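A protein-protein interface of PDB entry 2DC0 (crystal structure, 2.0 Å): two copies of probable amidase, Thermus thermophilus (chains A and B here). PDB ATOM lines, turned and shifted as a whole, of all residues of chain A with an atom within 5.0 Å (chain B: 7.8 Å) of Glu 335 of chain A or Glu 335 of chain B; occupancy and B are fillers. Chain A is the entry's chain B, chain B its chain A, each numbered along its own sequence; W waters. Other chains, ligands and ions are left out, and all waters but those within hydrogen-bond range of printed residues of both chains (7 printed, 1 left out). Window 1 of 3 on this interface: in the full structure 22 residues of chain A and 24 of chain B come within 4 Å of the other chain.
The guanidinium group (NH2) of Arg 338 of chain B lies close to the guanidinium group (NH2) of Arg 338 of chain A (3.3 Å).
NH2 of Arg 338 of chain B lies within salt-bridge range of OE2 of Glu 335 of chain A, 3.5 Å away.
The side-chain carboxylate (OE1) of Glu 335 of chain B is in salt-bridge range of the guanidinium group (NH2) of Arg 338 of chain A.
The side-chain carboxylate of Glu 335 of chain A is in salt-bridge range of the guanidinium group of Arg 338 of chain A (2.7 Å).
The guanidinium group of Arg 334 of chain B lies close to the backbone carbonyl oxygen of Leu 390 of chain B.
The side-chain hydroxyl (OG) of Ser 202 of chain B lies within hydrogen-bond range of the guanidinium group (NH2) of Arg 334 of chain B (3.1 Å).
Leu 339 of chain B touches Tyr 188 of chain A.
O of Ala 332 of chain A touches OH of Tyr 188 of chain B, 3.9 Å away.
NH2 of Arg 334 of chain A touches CG1 of Val 331 of chain B, 3.5 Å away.
Glu 335 of chain A touches Ser 202 of chain B (CG to O, 3.9 Å).
Tyr 416 of chain B touches Arg 338 of chain A.
Tyr 416 of chain B touches Leu 339 of chain A.
O of Glu 335 of chain B touches OH of Tyr 416 of chain A, at 3.8 Å.
Tyr 416 of chain A touches Arg 338 of chain B.
Glu 335 of chain A touches six residues of chain B.
Glu 335 of chain B touches just these residues of chain A: Tyr 188, Ser 202, Arg 334, Glu 335, Arg 338 and Tyr 416.
Of the printed residues of chain B, Arg 338 of chain A touches Glu 335, Arg 338 and Tyr 416.
Of the printed residues of chain A, Ala 336 of chain B touches Tyr 188.
Of the printed residues of chain B, Tyr 188 of chain A touches Ala 332 (3.9 Å), Glu 335 (3.4 Å), Ala 336 (3.6 Å) and Leu 339 (3.9 Å).
Of the printed residues of chain A, Tyr 416 of chain B touches Glu 335, Arg 338 and Leu 339.
Leu 288 of chain B touches none of the printed residues of chain A.
The nearest residue of chain B that does not touch Glu 335 of chain A is Leu 391 of chain B (5.3 Å).
Of the 25 printed residues of chain B, 10 touch a printed residue of chain A.
Printed residues of chain B that touch a printed residue of chain A: Tyr 188, Ser 202, Val 331, Ala 332, Arg 334, Glu 335, Ala 336, Arg 338, Leu 339 and Tyr 416.
Hydrophobic or aromatic side chains of chain B within 4 Å of the printed part of chain A: Tyr 188, Val 331, Leu 339 and Tyr 416.
Among the printed residues, 26 pairs touch across the chains.
Tyr 188 of chain A touches Glu 335 of chain B, and with the chains exchanged Glu 335 of chain A touches Tyr 188 of chain B.
Arg 338 of chain A touches its own counterpart, Arg 338 of chain B.
Of the 26 pairs that touch across the chains among the printed residues, 24 have their exchanged pair printed and touching as well.
Water W2 lies within hydrogen-bond range of O of Glu 335 of chain A (2.7 Å), OH of Tyr 416 of chain B (2.9 Å), N of Leu 339 of chain A (3.0 Å) and O of Ala 336 of chain A (3.5 Å).
Water W5 bridges OH of Tyr 188 of chain A (2.7 Å) and O of Ala 332 of chain B (3.1 Å).
Water W3 lies within hydrogen-bond range of the guanidinium group of Arg 338 of chain A (3.0 Å) and the side-chain carboxylate of Glu 335 of chain B (3.1 Å).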
ATOM      1  N   TYR A 188     -36.491 -21.438  -2.700  1.00  0.00           N
ATOM      2  CA  TYR A 188     -36.024 -20.057  -2.721  1.00  0.00           C
ATOM      3  C   TYR A 188     -34.915 -19.876  -3.763  1.00  0.00           C
ATOM      4  O   TYR A 188     -34.059 -20.744  -3.925  1.00  0.00           O
ATOM      5  CB  TYR A 188     -35.495 -19.656  -1.342  1.00  0.00           C
ATOM      6  CG  TYR A 188     -34.920 -18.254  -1.288  1.00  0.00           C
ATOM      7  CD1 TYR A 188     -35.725 -17.155  -0.985  1.00  0.00           C
ATOM      8  CD2 TYR A 188     -33.563 -18.029  -1.544  1.00  0.00           C
ATOM      9  CE1 TYR A 188     -35.191 -15.864  -0.931  1.00  0.00           C
ATOM     10  CE2 TYR A 188     -33.020 -16.746  -1.497  1.00  0.00           C
ATOM     11  CZ  TYR A 188     -33.838 -15.671  -1.188  1.00  0.00           C
ATOM     12  OH  TYR A 188     -33.297 -14.408  -1.118  1.00  0.00           O
ATOM     13  N   SER A 202     -34.638 -11.992   1.918  1.00  0.00           N
ATOM     14  CA  SER A 202     -34.173 -13.337   2.229  1.00  0.00           C
ATOM     15  C   SER A 202     -35.307 -14.337   2.381  1.00  0.00           C
ATOM     16  O   SER A 202     -35.073 -15.504   2.694  1.00  0.00           O
ATOM     17  CB  SER A 202     -33.306 -13.325   3.498  1.00  0.00           C
ATOM     18  OG  SER A 202     -34.072 -13.090   4.664  1.00  0.00           O
ATOM     19  N   VAL A 331     -32.300 -14.095  12.481  1.00  0.00           N
ATOM     20  CA  VAL A 331     -31.471 -14.764  11.486  1.00  0.00           C
ATOM     21  C   VAL A 331     -30.904 -16.055  12.074  1.00  0.00           C
ATOM     22  O   VAL A 331     -30.973 -17.122  11.453  1.00  0.00           O
ATOM     23  CB  VAL A 331     -30.305 -13.848  11.045  1.00  0.00           C
ATOM     24  CG1 VAL A 331     -29.308 -14.629  10.193  1.00  0.00           C
ATOM     25  CG2 VAL A 331     -30.848 -12.665  10.268  1.00  0.00           C
ATOM     26  N   ALA A 332     -30.345 -15.959  13.277  1.00  0.00           N
ATOM     27  CA  ALA A 332     -29.782 -17.133  13.935  1.00  0.00           C
ATOM     28  C   ALA A 332     -30.886 -18.140  14.267  1.00  0.00           C
ATOM     29  O   ALA A 332     -30.709 -19.339  14.083  1.00  0.00           O
ATOM     30  CB  ALA A 332     -29.035 -16.724  15.208  1.00  0.00           C
ATOM     31  N   GLU A 333     -32.025 -17.650  14.747  1.00  0.00           N
ATOM     32  CA  GLU A 333     -33.139 -18.534  15.091  1.00  0.00           C
ATOM     33  C   GLU A 333     -33.688 -19.284  13.867  1.00  0.00           C
ATOM     34  O   GLU A 333     -34.168 -20.414  13.991  1.00  0.00           O
ATOM     35  CB  GLU A 333     -34.264 -17.739  15.766  1.00  0.00           C
ATOM     36  CG  GLU A 333     -33.862 -17.095  17.096  1.00  0.00           C
ATOM     37  CD  GLU A 333     -34.982 -16.270  17.704  1.00  0.00           C
ATOM     38  OE1 GLU A 333     -35.599 -15.468  16.968  1.00  0.00           O
ATOM     39  OE2 GLU A 333     -35.238 -16.403  18.919  1.00  0.00           O
ATOM     40  N   ARG A 334     -33.633 -18.660  12.691  1.00  0.00           N
ATOM     41  CA  ARG A 334     -34.111 -19.326  11.474  1.00  0.00           C
ATOM     42  C   ARG A 334     -33.178 -20.490  11.152  1.00  0.00           C
ATOM     43  O   ARG A 334     -33.629 -21.595  10.844  1.00  0.00           O
ATOM     44  CB  ARG A 334     -34.151 -18.366  10.273  1.00  0.00           C
ATOM     45  CG  ARG A 334     -34.346 -19.104   8.934  1.00  0.00           C
ATOM     46  CD  ARG A 334     -34.706 -18.184   7.766  1.00  0.00           C
ATOM     47  NE  ARG A 334     -33.641 -17.250   7.411  1.00  0.00           N
ATOM     48  CZ  ARG A 334     -33.758 -16.319   6.466  1.00  0.00           C
ATOM     49  NH1 ARG A 334     -34.892 -16.204   5.785  1.00  0.00           N
ATOM     50  NH2 ARG A 334     -32.749 -15.496   6.206  1.00  0.00           N
ATOM     51  N   GLU A 335     -31.873 -20.238  11.207  1.00  0.00           N
ATOM     52  CA  GLU A 335     -30.908 -21.296  10.938  1.00  0.00           C
ATOM     53  C   GLU A 335     -31.101 -22.475  11.893  1.00  0.00           C
ATOM     54  O   GLU A 335     -30.910 -23.626  11.511  1.00  0.00           O
ATOM     55  CB  GLU A 335     -29.467 -20.774  11.057  1.00  0.00           C
ATOM     56  CG  GLU A 335     -29.057 -19.807   9.959  1.00  0.00           C
ATOM     57  CD  GLU A 335     -29.455 -20.302   8.578  1.00  0.00           C
ATOM     58  OE1 GLU A 335     -29.171 -21.479   8.264  1.00  0.00           O
ATOM     59  OE2 GLU A 335     -30.042 -19.509   7.809  1.00  0.00           O
ATOM     60  N   ALA A 336     -31.490 -22.189  13.132  1.00  0.00           N
ATOM     61  CA  ALA A 336     -31.685 -23.246  14.122  1.00  0.00           C
ATOM     62  C   ALA A 336     -32.879 -24.146  13.818  1.00  0.00           C
ATOM     63  O   ALA A 336     -32.912 -25.295  14.244  1.00  0.00           O
ATOM     64  CB  ALA A 336     -31.835 -22.644  15.510  1.00  0.00           C
ATOM     65  N   LEU A 337     -33.844 -23.628  13.067  1.00  0.00           N
ATOM     66  CA  LEU A 337     -35.037 -24.388  12.725  1.00  0.00           C
ATOM     67  C   LEU A 337     -34.869 -25.348  11.549  1.00  0.00           C
ATOM     68  O   LEU A 337     -35.641 -26.296  11.412  1.00  0.00           O
ATOM     69  CB  LEU A 337     -36.195 -23.426  12.426  1.00  0.00           C
ATOM     70  CG  LEU A 337     -36.684 -22.574  13.600  1.00  0.00           C
ATOM     71  CD1 LEU A 337     -37.652 -21.496  13.112  1.00  0.00           C
ATOM     72  CD2 LEU A 337     -37.350 -23.467  14.624  1.00  0.00           C
ATOM     73  N   ARG A 338     -33.868 -25.117  10.706  1.00  0.00           N
ATOM     74  CA  ARG A 338     -33.665 -25.970   9.536  1.00  0.00           C
ATOM     75  C   ARG A 338     -33.589 -27.463   9.808  1.00  0.00           C
ATOM     76  O   ARG A 338     -34.275 -28.246   9.150  1.00  0.00           O
ATOM     77  CB  ARG A 338     -32.411 -25.556   8.760  1.00  0.00           C
ATOM     78  CG  ARG A 338     -32.473 -24.178   8.168  1.00  0.00           C
ATOM     79  CD  ARG A 338     -31.324 -23.942   7.192  1.00  0.00           C
ATOM     80  NE  ARG A 338     -31.205 -22.525   6.875  1.00  0.00           N
ATOM     81  CZ  ARG A 338     -32.071 -21.846   6.134  1.00  0.00           C
ATOM     82  NH1 ARG A 338     -33.127 -22.462   5.619  1.00  0.00           N
ATOM     83  NH2 ARG A 338     -31.894 -20.545   5.935  1.00  0.00           N
ATOM     84  N   LEU A 339     -32.768 -27.873  10.770  1.00  0.00           N
ATOM     85  CA  LEU A 339     -32.632 -29.300  11.051  1.00  0.00           C
ATOM     86  C   LEU A 339     -33.973 -29.978  11.351  1.00  0.00           C
ATOM     87  O   LEU A 339     -34.208 -31.105  10.918  1.00  0.00           O
ATOM     88  CB  LEU A 339     -31.641 -29.532  12.200  1.00  0.00           C
ATOM     89  CG  LEU A 339     -31.231 -31.004  12.393  1.00  0.00           C
ATOM     90  CD1 LEU A 339     -30.673 -31.558  11.078  1.00  0.00           C
ATOM     91  CD2 LEU A 339     -30.193 -31.120  13.496  1.00  0.00           C
ATOM     92  N   TYR A 416     -35.637 -28.964   0.193  1.00  0.00           N
ATOM     93  CA  TYR A 416     -35.042 -27.897  -0.612  1.00  0.00           C
ATOM     94  C   TYR A 416     -34.545 -28.491  -1.930  1.00  0.00           C
ATOM     95  O   TYR A 416     -33.853 -29.508  -1.929  1.00  0.00           O
ATOM     96  CB  TYR A 416     -33.852 -27.290   0.139  1.00  0.00           C
ATOM     97  CG  TYR A 416     -33.653 -25.802  -0.063  1.00  0.00           C
ATOM     98  CD1 TYR A 416     -33.981 -24.899   0.946  1.00  0.00           C
ATOM     99  CD2 TYR A 416     -33.106 -25.299  -1.248  1.00  0.00           C
ATOM    100  CE1 TYR A 416     -33.766 -23.532   0.794  1.00  0.00           C
ATOM    101  CE2 TYR A 416     -32.891 -23.930  -1.415  1.00  0.00           C
ATOM    102  CZ  TYR A 416     -33.223 -23.053  -0.384  1.00  0.00           C
ATOM    103  OH  TYR A 416     -32.995 -21.697  -0.526  1.00  0.00           O
ATOM    104  N   TYR B 188     -25.237 -27.704  11.175  1.00  0.00           N
ATOM    105  CA  TYR B 188     -25.414 -26.562  12.063  1.00  0.00           C
ATOM    106  C   TYR B 188     -26.378 -26.889  13.205  1.00  0.00           C
ATOM    107  O   TYR B 188     -27.410 -27.526  12.988  1.00  0.00           O
ATOM    108  CB  TYR B 188     -25.958 -25.366  11.274  1.00  0.00           C
ATOM    109  CG  TYR B 188     -26.245 -24.149  12.123  1.00  0.00           C
ATOM    110  CD1 TYR B 188     -25.224 -23.269  12.485  1.00  0.00           C
ATOM    111  CD2 TYR B 188     -27.543 -23.874  12.565  1.00  0.00           C
ATOM    112  CE1 TYR B 188     -25.489 -22.144  13.263  1.00  0.00           C
ATOM    113  CE2 TYR B 188     -27.815 -22.751  13.346  1.00  0.00           C
ATOM    114  CZ  TYR B 188     -26.787 -21.893  13.689  1.00  0.00           C
ATOM    115  OH  TYR B 188     -27.061 -20.783  14.465  1.00  0.00           O
ATOM    116  N   GLY B 189     -26.017 -26.474  14.417  1.00  0.00           N
ATOM    117  CA  GLY B 189     -26.871 -26.678  15.571  1.00  0.00           C
ATOM    118  C   GLY B 189     -26.984 -28.054  16.197  1.00  0.00           C
ATOM    119  O   GLY B 189     -27.548 -28.179  17.284  1.00  0.00           O
ATOM    120  N   ARG B 201     -23.089 -16.245  15.483  1.00  0.00           N
ATOM    121  CA  ARG B 201     -24.132 -17.146  15.949  1.00  0.00           C
ATOM    122  C   ARG B 201     -24.851 -17.941  14.863  1.00  0.00           C
ATOM    123  O   ARG B 201     -25.236 -19.080  15.101  1.00  0.00           O
ATOM    124  CB  ARG B 201     -25.167 -16.376  16.772  1.00  0.00           C
ATOM    125  CG  ARG B 201     -24.664 -15.871  18.120  1.00  0.00           C
ATOM    126  CD  ARG B 201     -25.689 -14.936  18.743  1.00  0.00           C
ATOM    127  NE  ARG B 201     -26.984 -15.591  18.907  1.00  0.00           N
ATOM    128  CZ  ARG B 201     -28.146 -14.946  18.973  1.00  0.00           C
ATOM    129  NH1 ARG B 201     -28.178 -13.620  18.887  1.00  0.00           N
ATOM    130  NH2 ARG B 201     -29.275 -15.626  19.123  1.00  0.00           N
ATOM    131  N   SER B 202     -25.036 -17.361  13.678  1.00  0.00           N
ATOM    132  CA  SER B 202     -25.744 -18.071  12.614  1.00  0.00           C
ATOM    133  C   SER B 202     -24.817 -18.884  11.716  1.00  0.00           C
ATOM    134  O   SER B 202     -25.261 -19.479  10.732  1.00  0.00           O
ATOM    135  CB  SER B 202     -26.556 -17.089  11.756  1.00  0.00           C
ATOM    136  OG  SER B 202     -25.716 -16.248  10.988  1.00  0.00           O
ATOM    137  N   THR B 203     -23.535 -18.926  12.063  1.00  0.00           N
ATOM    138  CA  THR B 203     -22.574 -19.668  11.264  1.00  0.00           C
ATOM    139  C   THR B 203     -21.628 -20.537  12.095  1.00  0.00           C
ATOM    140  O   THR B 203     -20.955 -21.419  11.545  1.00  0.00           O
ATOM    141  CB  THR B 203     -21.744 -18.704  10.392  1.00  0.00           C
ATOM    142  OG1 THR B 203     -22.631 -17.814   9.701  1.00  0.00           O
ATOM    143  CG2 THR B 203     -20.933 -19.477   9.374  1.00  0.00           C
ATOM    144  N   VAL B 284     -19.443 -12.676   0.731  1.00  0.00           N
ATOM    145  CA  VAL B 284     -20.680 -12.867   1.485  1.00  0.00           C
ATOM    146  C   VAL B 284     -20.367 -13.364   2.892  1.00  0.00           C
ATOM    147  O   VAL B 284     -20.835 -12.801   3.884  1.00  0.00           O
ATOM    148  CB  VAL B 284     -21.625 -13.896   0.794  1.00  0.00           C
ATOM    149  CG1 VAL B 284     -22.824 -14.195   1.690  1.00  0.00           C
ATOM    150  CG2 VAL B 284     -22.110 -13.348  -0.544  1.00  0.00           C
ATOM    151  N   LEU B 288     -20.876 -11.178   6.430  1.00  0.00           N
ATOM    152  CA  LEU B 288     -21.837 -11.722   7.371  1.00  0.00           C
ATOM    153  C   LEU B 288     -21.201 -12.032   8.726  1.00  0.00           C
ATOM    154  O   LEU B 288     -21.713 -11.622   9.763  1.00  0.00           O
ATOM    155  CB  LEU B 288     -22.486 -12.981   6.779  1.00  0.00           C
ATOM    156  CG  LEU B 288     -23.780 -13.432   7.461  1.00  0.00           C
ATOM    157  CD1 LEU B 288     -24.591 -14.341   6.542  1.00  0.00           C
ATOM    158  CD2 LEU B 288     -23.427 -14.139   8.757  1.00  0.00           C
ATOM    159  N   GLU B 292     -21.516  -9.881  12.472  1.00  0.00           N
ATOM    160  CA  GLU B 292     -21.988 -10.514  13.705  1.00  0.00           C
ATOM    161  C   GLU B 292     -20.912 -10.525  14.784  1.00  0.00           C
ATOM    162  O   GLU B 292     -21.202 -10.261  15.953  1.00  0.00           O
ATOM    163  CB  GLU B 292     -22.469 -11.958  13.444  1.00  0.00           C
ATOM    164  CG  GLU B 292     -23.691 -12.070  12.524  1.00  0.00           C
ATOM    165  CD  GLU B 292     -24.303 -13.478  12.487  1.00  0.00           C
ATOM    166  OE1 GLU B 292     -23.682 -14.436  12.992  1.00  0.00           O
ATOM    167  OE2 GLU B 292     -25.413 -13.625  11.937  1.00  0.00           O
ATOM    168  N   ASP B 329     -28.097  -7.665   3.177  1.00  0.00           N
ATOM    169  CA  ASP B 329     -27.678  -8.115   1.848  1.00  0.00           C
ATOM    170  C   ASP B 329     -26.916  -9.433   1.959  1.00  0.00           C
ATOM    171  O   ASP B 329     -27.128 -10.361   1.167  1.00  0.00           O
ATOM    172  CB  ASP B 329     -26.776  -7.072   1.171  1.00  0.00           C
ATOM    173  CG  ASP B 329     -27.534  -5.823   0.748  1.00  0.00           C
ATOM    174  OD1 ASP B 329     -28.774  -5.883   0.641  1.00  0.00           O
ATOM    175  OD2 ASP B 329     -26.882  -4.785   0.508  1.00  0.00           O
ATOM    176  N   ALA B 330     -26.021  -9.508   2.942  1.00  0.00           N
ATOM    177  CA  ALA B 330     -25.239 -10.719   3.159  1.00  0.00           C
ATOM    178  C   ALA B 330     -26.180 -11.878   3.474  1.00  0.00           C
ATOM    179  O   ALA B 330     -26.006 -12.982   2.964  1.00  0.00           O
ATOM    180  CB  ALA B 330     -24.252 -10.508   4.312  1.00  0.00           C
ATOM    181  N   VAL B 331     -27.174 -11.616   4.321  1.00  0.00           N
ATOM    182  CA  VAL B 331     -28.153 -12.632   4.705  1.00  0.00           C
ATOM    183  C   VAL B 331     -28.934 -13.140   3.483  1.00  0.00           C
ATOM    184  O   VAL B 331     -29.195 -14.338   3.354  1.00  0.00           O
ATOM    185  CB  VAL B 331     -29.142 -12.075   5.757  1.00  0.00           C
ATOM    186  CG1 VAL B 331     -30.299 -13.044   5.969  1.00  0.00           C
ATOM    187  CG2 VAL B 331     -28.404 -11.844   7.078  1.00  0.00           C
ATOM    188  N   ALA B 332     -29.302 -12.223   2.593  1.00  0.00           N
ATOM    189  CA  ALA B 332     -30.039 -12.581   1.390  1.00  0.00           C
ATOM    190  C   ALA B 332     -29.125 -13.315   0.404  1.00  0.00           C
ATOM    191  O   ALA B 332     -29.546 -14.267  -0.250  1.00  0.00           O
ATOM    192  CB  ALA B 332     -30.626 -11.318   0.731  1.00  0.00           C
ATOM    193  N   GLU B 333     -27.882 -12.864   0.291  1.00  0.00           N
ATOM    194  CA  GLU B 333     -26.935 -13.497  -0.617  1.00  0.00           C
ATOM    195  C   GLU B 333     -26.636 -14.928  -0.179  1.00  0.00           C
ATOM    196  O   GLU B 333     -26.391 -15.799  -1.019  1.00  0.00           O
ATOM    197  CB  GLU B 333     -25.631 -12.694  -0.697  1.00  0.00           C
ATOM    198  CG  GLU B 333     -25.762 -11.343  -1.399  1.00  0.00           C
ATOM    199  CD  GLU B 333     -26.372 -11.457  -2.791  1.00  0.00           C
ATOM    200  OE1 GLU B 333     -25.927 -12.324  -3.576  1.00  0.00           O
ATOM    201  OE2 GLU B 333     -27.297 -10.673  -3.108  1.00  0.00           O
ATOM    202  N   ARG B 334     -26.650 -15.178   1.128  1.00  0.00           N
ATOM    203  CA  ARG B 334     -26.398 -16.527   1.623  1.00  0.00           C
ATOM    204  C   ARG B 334     -27.533 -17.443   1.202  1.00  0.00           C
ATOM    205  O   ARG B 334     -27.300 -18.562   0.763  1.00  0.00           O
ATOM    206  CB  ARG B 334     -26.270 -16.559   3.155  1.00  0.00           C
ATOM    207  CG  ARG B 334     -26.366 -17.983   3.709  1.00  0.00           C
ATOM    208  CD  ARG B 334     -25.826 -18.125   5.126  1.00  0.00           C
ATOM    209  NE  ARG B 334     -26.630 -17.449   6.137  1.00  0.00           N
ATOM    210  CZ  ARG B 334     -26.327 -17.445   7.431  1.00  0.00           C
ATOM    211  NH1 ARG B 334     -25.241 -18.083   7.858  1.00  0.00           N
ATOM    212  NH2 ARG B 334     -27.097 -16.798   8.297  1.00  0.00           N
ATOM    213  N   GLU B 335     -28.768 -16.972   1.346  1.00  0.00           N
ATOM    214  CA  GLU B 335     -29.906 -17.794   0.965  1.00  0.00           C
ATOM    215  C   GLU B 335     -29.872 -18.085  -0.533  1.00  0.00           C
ATOM    216  O   GLU B 335     -30.222 -19.181  -0.966  1.00  0.00           O
ATOM    217  CB  GLU B 335     -31.223 -17.111   1.364  1.00  0.00           C
ATOM    218  CG  GLU B 335     -31.426 -17.042   2.891  1.00  0.00           C
ATOM    219  CD  GLU B 335     -31.102 -18.368   3.578  1.00  0.00           C
ATOM    220  OE1 GLU B 335     -31.704 -19.405   3.199  1.00  0.00           O
ATOM    221  OE2 GLU B 335     -30.243 -18.376   4.495  1.00  0.00           O
ATOM    222  N   ALA B 336     -29.428 -17.111  -1.320  1.00  0.00           N
ATOM    223  CA  ALA B 336     -29.346 -17.287  -2.767  1.00  0.00           C
ATOM    224  C   ALA B 336     -28.374 -18.403  -3.171  1.00  0.00           C
ATOM    225  O   ALA B 336     -28.519 -18.991  -4.237  1.00  0.00           O
ATOM    226  CB  ALA B 336     -28.933 -15.970  -3.429  1.00  0.00           C
ATOM    227  N   LEU B 337     -27.393 -18.696  -2.322  1.00  0.00           N
ATOM    228  CA  LEU B 337     -26.407 -19.732  -2.623  1.00  0.00           C
ATOM    229  C   LEU B 337     -26.843 -21.130  -2.204  1.00  0.00           C
ATOM    230  O   LEU B 337     -26.312 -22.130  -2.695  1.00  0.00           O
ATOM    231  CB  LEU B 337     -25.083 -19.414  -1.931  1.00  0.00           C
ATOM    232  CG  LEU B 337     -24.361 -18.141  -2.387  1.00  0.00           C
ATOM    233  CD1 LEU B 337     -23.263 -17.793  -1.395  1.00  0.00           C
ATOM    234  CD2 LEU B 337     -23.792 -18.349  -3.778  1.00  0.00           C
ATOM    235  N   ARG B 338     -27.807 -21.193  -1.294  1.00  0.00           N
ATOM    236  CA  ARG B 338     -28.291 -22.462  -0.774  1.00  0.00           C
ATOM    237  C   ARG B 338     -28.753 -23.442  -1.853  1.00  0.00           C
ATOM    238  O   ARG B 338     -28.384 -24.616  -1.815  1.00  0.00           O
ATOM    239  CB  ARG B 338     -29.410 -22.201   0.248  1.00  0.00           C
ATOM    240  CG  ARG B 338     -29.630 -23.339   1.233  1.00  0.00           C
ATOM    241  CD  ARG B 338     -30.594 -22.943   2.354  1.00  0.00           C
ATOM    242  NE  ARG B 338     -30.119 -21.809   3.147  1.00  0.00           N
ATOM    243  CZ  ARG B 338     -29.201 -21.882   4.109  1.00  0.00           C
ATOM    244  NH1 ARG B 338     -28.638 -23.043   4.418  1.00  0.00           N
ATOM    245  NH2 ARG B 338     -28.850 -20.788   4.775  1.00  0.00           N
ATOM    246  N   LEU B 339     -29.533 -22.974  -2.827  1.00  0.00           N
ATOM    247  CA  LEU B 339     -30.018 -23.871  -3.883  1.00  0.00           C
ATOM    248  C   LEU B 339     -28.871 -24.477  -4.701  1.00  0.00           C
ATOM    249  O   LEU B 339     -28.953 -25.629  -5.140  1.00  0.00           O
ATOM    250  CB  LEU B 339     -31.000 -23.139  -4.813  1.00  0.00           C
ATOM    251  CG  LEU B 339     -31.666 -23.961  -5.923  1.00  0.00           C
ATOM    252  CD1 LEU B 339     -32.406 -25.160  -5.328  1.00  0.00           C
ATOM    253  CD2 LEU B 339     -32.633 -23.074  -6.706  1.00  0.00           C
ATOM    254  N   GLU B 340     -27.803 -23.705  -4.898  1.00  0.00           N
ATOM    255  CA  GLU B 340     -26.634 -24.174  -5.651  1.00  0.00           C
ATOM    256  C   GLU B 340     -25.978 -25.391  -5.007  1.00  0.00           C
ATOM    257  O   GLU B 340     -25.575 -26.334  -5.694  1.00  0.00           O
ATOM    258  CB  GLU B 340     -25.576 -23.073  -5.759  1.00  0.00           C
ATOM    259  CG  GLU B 340     -25.790 -22.092  -6.882  1.00  0.00           C
ATOM    260  CD  GLU B 340     -24.615 -21.149  -7.037  1.00  0.00           C
ATOM    261  OE1 GLU B 340     -23.461 -21.630  -7.006  1.00  0.00           O
ATOM    262  OE2 GLU B 340     -24.848 -19.933  -7.195  1.00  0.00           O
ATOM    263  N   SER B 389     -19.684 -24.348   5.997  1.00  0.00           N
ATOM    264  CA  SER B 389     -20.015 -23.893   7.337  1.00  0.00           C
ATOM    265  C   SER B 389     -21.034 -22.761   7.156  1.00  0.00           C
ATOM    266  O   SER B 389     -22.000 -22.650   7.913  1.00  0.00           O
ATOM    267  CB  SER B 389     -18.767 -23.385   8.068  1.00  0.00           C
ATOM    268  OG  SER B 389     -18.001 -22.533   7.240  1.00  0.00           O
ATOM    269  N   LEU B 390     -20.820 -21.934   6.136  1.00  0.00           N
ATOM    270  CA  LEU B 390     -21.732 -20.832   5.839  1.00  0.00           C
ATOM    271  C   LEU B 390     -23.152 -21.367   5.672  1.00  0.00           C
ATOM    272  O   LEU B 390     -24.107 -20.777   6.179  1.00  0.00           O
ATOM    273  CB  LEU B 390     -21.321 -20.117   4.542  1.00  0.00           C
ATOM    274  CG  LEU B 390     -22.265 -18.991   4.081  1.00  0.00           C
ATOM    275  CD1 LEU B 390     -22.201 -17.820   5.057  1.00  0.00           C
ATOM    276  CD2 LEU B 390     -21.879 -18.533   2.679  1.00  0.00           C
ATOM    277  N   LEU B 391     -23.278 -22.489   4.968  1.00  0.00           N
ATOM    278  CA  LEU B 391     -24.580 -23.096   4.699  1.00  0.00           C
ATOM    279  C   LEU B 391     -25.011 -24.190   5.684  1.00  0.00           C
ATOM    280  O   LEU B 391     -26.086 -24.765   5.538  1.00  0.00           O
ATOM    281  CB  LEU B 391     -24.613 -23.620   3.256  1.00  0.00           C
ATOM    282  CG  LEU B 391     -24.441 -22.508   2.204  1.00  0.00           C
ATOM    283  CD1 LEU B 391     -24.372 -23.095   0.791  1.00  0.00           C
ATOM    284  CD2 LEU B 391     -25.624 -21.543   2.311  1.00  0.00           C
ATOM    285  N   GLY B 392     -24.165 -24.475   6.673  1.00  0.00           N
ATOM    286  CA  GLY B 392     -24.500 -25.445   7.710  1.00  0.00           C
ATOM    287  C   GLY B 392     -24.528 -26.945   7.458  1.00  0.00           C
ATOM    288  O   GLY B 392     -25.046 -27.689   8.298  1.00  0.00           O
ATOM    289  N   TYR B 416     -27.568 -31.470   4.246  1.00  0.00           N
ATOM    290  CA  TYR B 416     -27.953 -30.992   5.563  1.00  0.00           C
ATOM    291  C   TYR B 416     -28.584 -32.143   6.354  1.00  0.00           C
ATOM    292  O   TYR B 416     -29.450 -32.853   5.844  1.00  0.00           O
ATOM    293  CB  TYR B 416     -28.948 -29.839   5.402  1.00  0.00           C
ATOM    294  CG  TYR B 416     -28.918 -28.817   6.517  1.00  0.00           C
ATOM    295  CD1 TYR B 416     -28.370 -27.549   6.322  1.00  0.00           C
ATOM    296  CD2 TYR B 416     -29.444 -29.116   7.767  1.00  0.00           C
ATOM    297  CE1 TYR B 416     -28.350 -26.603   7.353  1.00  0.00           C
ATOM    298  CE2 TYR B 416     -29.428 -28.184   8.801  1.00  0.00           C
ATOM    299  CZ  TYR B 416     -28.881 -26.933   8.585  1.00  0.00           C
ATOM    300  OH  TYR B 416     -28.877 -26.026   9.612  1.00  0.00           O
HETATM  301  O   HOH W   1     -27.700 -23.620   9.015  1.00  0.00           O
HETATM  302  O   HOH W   2     -30.509 -26.272  11.948  1.00  0.00           O
HETATM  303  O   HOH W   3     -34.473 -20.077   4.399  1.00  0.00           O
HETATM  304  O   HOH W   4     -29.133 -20.434  16.314  1.00  0.00           O
HETATM  305  O   HOH W   5     -31.295 -13.414  -2.669  1.00  0.00           O
HETATM  306  O   HOH W   6     -30.092 -27.209  14.419  1.00  0.00           O
HETATM  307  O   HOH W   7     -33.816 -20.111   1.639  1.00  0.00           O
